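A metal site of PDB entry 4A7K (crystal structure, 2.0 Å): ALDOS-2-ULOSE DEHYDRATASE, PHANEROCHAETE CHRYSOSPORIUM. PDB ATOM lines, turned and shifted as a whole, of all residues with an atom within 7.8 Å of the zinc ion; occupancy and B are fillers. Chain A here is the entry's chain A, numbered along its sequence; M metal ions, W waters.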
ATOM      1  N   GLY A 628     -11.216   6.655  -8.555  1.00  0.00           N
ATOM      2  CA  GLY A 628     -10.449   5.573  -7.967  1.00  0.00           C
ATOM      3  C   GLY A 628     -10.972   4.167  -8.304  1.00  0.00           C
ATOM      4  O   GLY A 628     -12.204   3.827  -8.145  1.00  0.00           O
ATOM      5  N   PHE A 629     -10.022   3.313  -8.751  1.00  0.00           N
ATOM      6  CA  PHE A 629     -10.350   1.898  -9.057  1.00  0.00           C
ATOM      7  C   PHE A 629     -10.736   1.086  -7.821  1.00  0.00           C
ATOM      8  O   PHE A 629     -10.064   1.177  -6.785  1.00  0.00           O
ATOM      9  CB  PHE A 629      -9.180   1.272  -9.819  1.00  0.00           C
ATOM     10  CG  PHE A 629      -9.129   1.681 -11.244  1.00  0.00           C
ATOM     11  CD1 PHE A 629      -9.862   0.988 -12.180  1.00  0.00           C
ATOM     12  CD2 PHE A 629      -8.411   2.830 -11.639  1.00  0.00           C
ATOM     13  CE1 PHE A 629      -9.852   1.377 -13.511  1.00  0.00           C
ATOM     14  CE2 PHE A 629      -8.408   3.228 -12.949  1.00  0.00           C
ATOM     15  CZ  PHE A 629      -9.141   2.502 -13.903  1.00  0.00           C
ATOM     16  N   HIS A 630     -11.822   0.310  -7.915  1.00  0.00           N
ATOM     17  CA  HIS A 630     -12.315  -0.467  -6.747  1.00  0.00           C
ATOM     18  C   HIS A 630     -13.075  -1.611  -7.349  1.00  0.00           C
ATOM     19  O   HIS A 630     -13.190  -1.724  -8.598  1.00  0.00           O
ATOM     20  CB  HIS A 630     -13.200   0.437  -5.856  1.00  0.00           C
ATOM     21  CG  HIS A 630     -14.388   0.960  -6.601  1.00  0.00           C
ATOM     22  ND1 HIS A 630     -14.314   2.034  -7.445  1.00  0.00           N
ATOM     23  CD2 HIS A 630     -15.654   0.433  -6.760  1.00  0.00           C
ATOM     24  CE1 HIS A 630     -15.504   2.197  -8.063  1.00  0.00           C
ATOM     25  NE2 HIS A 630     -16.325   1.225  -7.625  1.00  0.00           N
ATOM     26  N   ASN A 631     -13.568  -2.506  -6.490  1.00  0.00           N
ATOM     27  CA  ASN A 631     -14.179  -3.766  -6.953  1.00  0.00           C
ATOM     28  C   ASN A 631     -15.305  -4.276  -6.080  1.00  0.00           C
ATOM     29  O   ASN A 631     -15.786  -5.386  -6.311  1.00  0.00           O
ATOM     30  CB  ASN A 631     -13.116  -4.875  -7.135  1.00  0.00           C
ATOM     31  CG  ASN A 631     -12.557  -5.392  -5.780  1.00  0.00           C
ATOM     32  OD1 ASN A 631     -12.833  -4.812  -4.705  1.00  0.00           O
ATOM     33  ND2 ASN A 631     -11.712  -6.402  -5.839  1.00  0.00           N
ATOM     34  N   HIS A 632     -15.757  -3.494  -5.084  1.00  0.00           N
ATOM     35  CA  HIS A 632     -16.960  -3.862  -4.265  1.00  0.00           C
ATOM     36  C   HIS A 632     -16.842  -5.161  -3.518  1.00  0.00           C
ATOM     37  O   HIS A 632     -17.855  -5.912  -3.381  1.00  0.00           O
ATOM     38  CB  HIS A 632     -18.299  -3.828  -5.103  1.00  0.00           C
ATOM     39  CG  HIS A 632     -18.495  -2.502  -5.766  1.00  0.00           C
ATOM     40  ND1 HIS A 632     -18.624  -1.342  -5.037  1.00  0.00           N
ATOM     41  CD2 HIS A 632     -18.495  -2.136  -7.123  1.00  0.00           C
ATOM     42  CE1 HIS A 632     -18.728  -0.300  -5.944  1.00  0.00           C
ATOM     43  NE2 HIS A 632     -18.652  -0.804  -7.191  1.00  0.00           N
ATOM     44  N   PHE A 637     -23.395  -5.456  -4.247  1.00  0.00           N
ATOM     45  CA  PHE A 637     -24.543  -4.954  -4.997  1.00  0.00           C
ATOM     46  C   PHE A 637     -24.250  -4.885  -6.524  1.00  0.00           C
ATOM     47  O   PHE A 637     -23.115  -5.039  -6.906  1.00  0.00           O
ATOM     48  CB  PHE A 637     -24.992  -3.591  -4.436  1.00  0.00           C
ATOM     49  CG  PHE A 637     -23.853  -2.551  -4.336  1.00  0.00           C
ATOM     50  CD1 PHE A 637     -23.300  -1.970  -5.483  1.00  0.00           C
ATOM     51  CD2 PHE A 637     -23.386  -2.150  -3.095  1.00  0.00           C
ATOM     52  CE1 PHE A 637     -22.283  -1.036  -5.363  1.00  0.00           C
ATOM     53  CE2 PHE A 637     -22.379  -1.196  -2.974  1.00  0.00           C
ATOM     54  CZ  PHE A 637     -21.809  -0.673  -4.097  1.00  0.00           C
ATOM     55  N   GLU A 639     -24.351  -2.498  -9.580  1.00  0.00           N
ATOM     56  CA  GLU A 639     -24.486  -1.043  -9.767  1.00  0.00           C
ATOM     57  C   GLU A 639     -24.587  -0.608 -11.215  1.00  0.00           C
ATOM     58  O   GLU A 639     -23.931  -1.135 -12.138  1.00  0.00           O
ATOM     59  CB  GLU A 639     -23.351  -0.249  -9.060  1.00  0.00           C
ATOM     60  CG  GLU A 639     -21.965  -0.575  -9.520  1.00  0.00           C
ATOM     61  CD  GLU A 639     -20.897   0.415  -9.059  1.00  0.00           C
ATOM     62  OE1 GLU A 639     -21.102   1.208  -8.108  1.00  0.00           O
ATOM     63  OE2 GLU A 639     -19.787   0.371  -9.679  1.00  0.00           O
ATOM     64  N   HIS A 641     -24.631   3.218 -13.392  1.00  0.00           N
ATOM     65  CA  HIS A 641     -24.506   4.659 -13.278  1.00  0.00           C
ATOM     66  C   HIS A 641     -25.206   5.322 -14.429  1.00  0.00           C
ATOM     67  O   HIS A 641     -25.168   4.829 -15.534  1.00  0.00           O
ATOM     68  CB  HIS A 641     -23.035   5.088 -13.261  1.00  0.00           C
ATOM     69  CG  HIS A 641     -22.241   4.489 -12.125  1.00  0.00           C
ATOM     70  ND1 HIS A 641     -21.409   3.452 -12.303  1.00  0.00           N
ATOM     71  CD2 HIS A 641     -22.221   4.786 -10.763  1.00  0.00           C
ATOM     72  CE1 HIS A 641     -20.849   3.117 -11.121  1.00  0.00           C
ATOM     73  NE2 HIS A 641     -21.310   3.943 -10.187  1.00  0.00           N
ATOM     74  N   MET A 653     -16.655   5.275 -17.668  1.00  0.00           N
ATOM     75  CA  MET A 653     -16.217   4.094 -16.891  1.00  0.00           C
ATOM     76  C   MET A 653     -15.101   3.364 -17.586  1.00  0.00           C
ATOM     77  O   MET A 653     -15.138   3.127 -18.807  1.00  0.00           O
ATOM     78  CB  MET A 653     -17.387   3.136 -16.643  1.00  0.00           C
ATOM     79  CG  MET A 653     -18.552   3.829 -15.887  1.00  0.00           C
ATOM     80  SD  MET A 653     -18.171   4.217 -14.151  1.00  0.00           S
ATOM     81  CE  MET A 653     -17.825   2.636 -13.384  1.00  0.00           C
ATOM     82  N   HIS A 684     -24.969   3.412 -18.370  1.00  0.00           N
ATOM     83  CA  HIS A 684     -24.092   2.355 -18.977  1.00  0.00           C
ATOM     84  C   HIS A 684     -24.606   1.006 -18.487  1.00  0.00           C
ATOM     85  O   HIS A 684     -25.314   0.972 -17.496  1.00  0.00           O
ATOM     86  CB  HIS A 684     -22.608   2.568 -18.639  1.00  0.00           C
ATOM     87  CG  HIS A 684     -22.303   2.249 -17.182  1.00  0.00           C
ATOM     88  ND1 HIS A 684     -22.273   0.980 -16.707  1.00  0.00           N
ATOM     89  CD2 HIS A 684     -22.057   3.078 -16.093  1.00  0.00           C
ATOM     90  CE1 HIS A 684     -22.018   0.993 -15.382  1.00  0.00           C
ATOM     91  NE2 HIS A 684     -21.861   2.285 -15.004  1.00  0.00           N
ATOM     92  N   LEU A 687     -20.974  -3.898 -15.458  1.00  0.00           N
ATOM     93  CA  LEU A 687     -19.561  -4.179 -15.641  1.00  0.00           C
ATOM     94  C   LEU A 687     -19.147  -5.322 -14.719  1.00  0.00           C
ATOM     95  O   LEU A 687     -18.011  -5.783 -14.771  1.00  0.00           O
ATOM     96  CB  LEU A 687     -18.741  -2.956 -15.317  1.00  0.00           C
ATOM     97  CG  LEU A 687     -19.156  -1.678 -16.003  1.00  0.00           C
ATOM     98  CD1 LEU A 687     -18.284  -0.508 -15.519  1.00  0.00           C
ATOM     99  CD2 LEU A 687     -19.015  -1.847 -17.508  1.00  0.00           C
ATOM    100  N   TYR A 706     -16.541  -7.998  -9.352  1.00  0.00           N
ATOM    101  CA  TYR A 706     -16.290  -6.993 -10.381  1.00  0.00           C
ATOM    102  C   TYR A 706     -14.842  -7.023 -10.728  1.00  0.00           C
ATOM    103  O   TYR A 706     -13.983  -7.275  -9.822  1.00  0.00           O
ATOM    104  CB  TYR A 706     -16.513  -5.601  -9.829  1.00  0.00           C
ATOM    105  CG  TYR A 706     -17.953  -5.217  -9.613  1.00  0.00           C
ATOM    106  CD1 TYR A 706     -18.687  -5.753  -8.513  1.00  0.00           C
ATOM    107  CD2 TYR A 706     -18.562  -4.292 -10.437  1.00  0.00           C
ATOM    108  CE1 TYR A 706     -19.997  -5.338  -8.257  1.00  0.00           C
ATOM    109  CE2 TYR A 706     -19.883  -3.879 -10.216  1.00  0.00           C
ATOM    110  CZ  TYR A 706     -20.614  -4.454  -9.168  1.00  0.00           C
ATOM    111  OH  TYR A 706     -21.900  -3.983  -8.919  1.00  0.00           O
ATOM    112  N   PRO A 707     -14.510  -6.788 -12.016  1.00  0.00           N
ATOM    113  CA  PRO A 707     -13.135  -6.426 -12.313  1.00  0.00           C
ATOM    114  C   PRO A 707     -12.878  -5.034 -11.691  1.00  0.00           C
ATOM    115  O   PRO A 707     -13.839  -4.349 -11.298  1.00  0.00           O
ATOM    116  CB  PRO A 707     -13.163  -6.312 -13.829  1.00  0.00           C
ATOM    117  CG  PRO A 707     -14.544  -5.720 -14.103  1.00  0.00           C
ATOM    118  CD  PRO A 707     -15.430  -6.467 -13.144  1.00  0.00           C
ATOM    119  N   TRP A 708     -11.603  -4.651 -11.525  1.00  0.00           N
ATOM    120  CA  TRP A 708     -11.276  -3.307 -11.082  1.00  0.00           C
ATOM    121  C   TRP A 708     -11.904  -2.344 -12.067  1.00  0.00           C
ATOM    122  O   TRP A 708     -11.802  -2.542 -13.294  1.00  0.00           O
ATOM    123  CB  TRP A 708      -9.743  -3.122 -11.106  1.00  0.00           C
ATOM    124  CG  TRP A 708      -8.967  -3.951 -10.102  1.00  0.00           C
ATOM    125  CD1 TRP A 708      -8.038  -4.963 -10.347  1.00  0.00           C
ATOM    126  CD2 TRP A 708      -8.982  -3.775  -8.640  1.00  0.00           C
ATOM    127  NE1 TRP A 708      -7.524  -5.436  -9.175  1.00  0.00           N
ATOM    128  CE2 TRP A 708      -8.042  -4.745  -8.104  1.00  0.00           C
ATOM    129  CE3 TRP A 708      -9.662  -2.916  -7.766  1.00  0.00           C
ATOM    130  CZ2 TRP A 708      -7.814  -4.856  -6.736  1.00  0.00           C
ATOM    131  CZ3 TRP A 708      -9.430  -3.061  -6.386  1.00  0.00           C
ATOM    132  CH2 TRP A 708      -8.529  -4.004  -5.898  1.00  0.00           C
ATOM    133  N   HIS A 709     -12.508  -1.264 -11.559  1.00  0.00           N
ATOM    134  CA  HIS A 709     -13.242  -0.303 -12.429  1.00  0.00           C
ATOM    135  C   HIS A 709     -13.361   1.043 -11.702  1.00  0.00           C
ATOM    136  O   HIS A 709     -13.166   1.131 -10.489  1.00  0.00           O
ATOM    137  CB  HIS A 709     -14.636  -0.838 -12.856  1.00  0.00           C
ATOM    138  CG  HIS A 709     -15.565  -1.015 -11.688  1.00  0.00           C
ATOM    139  ND1 HIS A 709     -15.413  -2.028 -10.806  1.00  0.00           N
ATOM    140  CD2 HIS A 709     -16.523  -0.167 -11.146  1.00  0.00           C
ATOM    141  CE1 HIS A 709     -16.305  -1.883  -9.772  1.00  0.00           C
ATOM    142  NE2 HIS A 709     -16.975  -0.749  -9.973  1.00  0.00           N
ATOM    143  N   ALA A 710     -13.638   2.128 -12.448  1.00  0.00           N
ATOM    144  CA  ALA A 710     -13.702   3.446 -11.859  1.00  0.00           C
ATOM    145  C   ALA A 710     -14.394   4.341 -12.849  1.00  0.00           C
ATOM    146  O   ALA A 710     -14.346   4.068 -14.056  1.00  0.00           O
ATOM    147  CB  ALA A 710     -12.283   3.961 -11.603  1.00  0.00           C
ATOM    148  N   TRP A 711     -15.068   5.401 -12.361  1.00  0.00           N
ATOM    149  CA  TRP A 711     -15.416   6.554 -13.202  1.00  0.00           C
ATOM    150  C   TRP A 711     -14.151   7.396 -13.245  1.00  0.00           C
ATOM    151  O   TRP A 711     -13.549   7.649 -12.167  1.00  0.00           O
ATOM    152  CB  TRP A 711     -16.625   7.373 -12.618  1.00  0.00           C
ATOM    153  CG  TRP A 711     -16.969   8.570 -13.502  1.00  0.00           C
ATOM    154  CD1 TRP A 711     -16.246   9.763 -13.676  1.00  0.00           C
ATOM    155  CD2 TRP A 711     -18.087   8.670 -14.462  1.00  0.00           C
ATOM    156  NE1 TRP A 711     -16.831  10.577 -14.643  1.00  0.00           N
ATOM    157  CE2 TRP A 711     -17.950   9.960 -15.138  1.00  0.00           C
ATOM    158  CE3 TRP A 711     -19.159   7.830 -14.791  1.00  0.00           C
ATOM    159  CZ2 TRP A 711     -18.877  10.384 -16.108  1.00  0.00           C
ATOM    160  CZ3 TRP A 711     -20.075   8.280 -15.788  1.00  0.00           C
ATOM    161  CH2 TRP A 711     -19.918   9.512 -16.411  1.00  0.00           C
ATOM    162  N   ALA A 728     -25.386   7.049  -8.939  1.00  0.00           N
ATOM    163  CA  ALA A 728     -25.230   5.606  -8.717  1.00  0.00           C
ATOM    164  C   ALA A 728     -26.558   4.936  -8.280  1.00  0.00           C
ATOM    165  O   ALA A 728     -27.229   5.416  -7.351  1.00  0.00           O
ATOM    166  CB  ALA A 728     -24.141   5.303  -7.707  1.00  0.00           C
HETATM  167 ZN    ZN M   1     -18.058   0.585  -8.680  1.00  0.00          ZN
HETATM  168  O   HOH W   1     -18.066   2.639  -9.894  1.00  0.00           O
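OE1 of Glu 639 sits at hydrogen-bond distance from NE2 of His 641. The side-chain hydroxyl (OH) of Tyr 706 sits at hydrogen-bond distance from the backbone NH (N) of Glu 639. ND1 of His 630 lies within hydrogen-bond range of O of Gly 628, at 2.9 Å. The backbone carbonyl oxygen of Pro 707 lies within hydrogen-bond range of a ring nitrogen (ND1) of His 709 (2.8 Å).
Four residues have an atom within 4 Å of the zinc ion: His 630, His 632, Glu 639 and His 709.
The zinc ion is bound by the side-chain carboxylate of Glu 639 (2.0 Å), a ring nitrogen (NE2) of His 632 (2.1 Å), a ring nitrogen (NE2) of His 630 (2.1 Å), a ring nitrogen (NE2) of His 709 (2.2 Å) and water W1 (2.4 Å).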
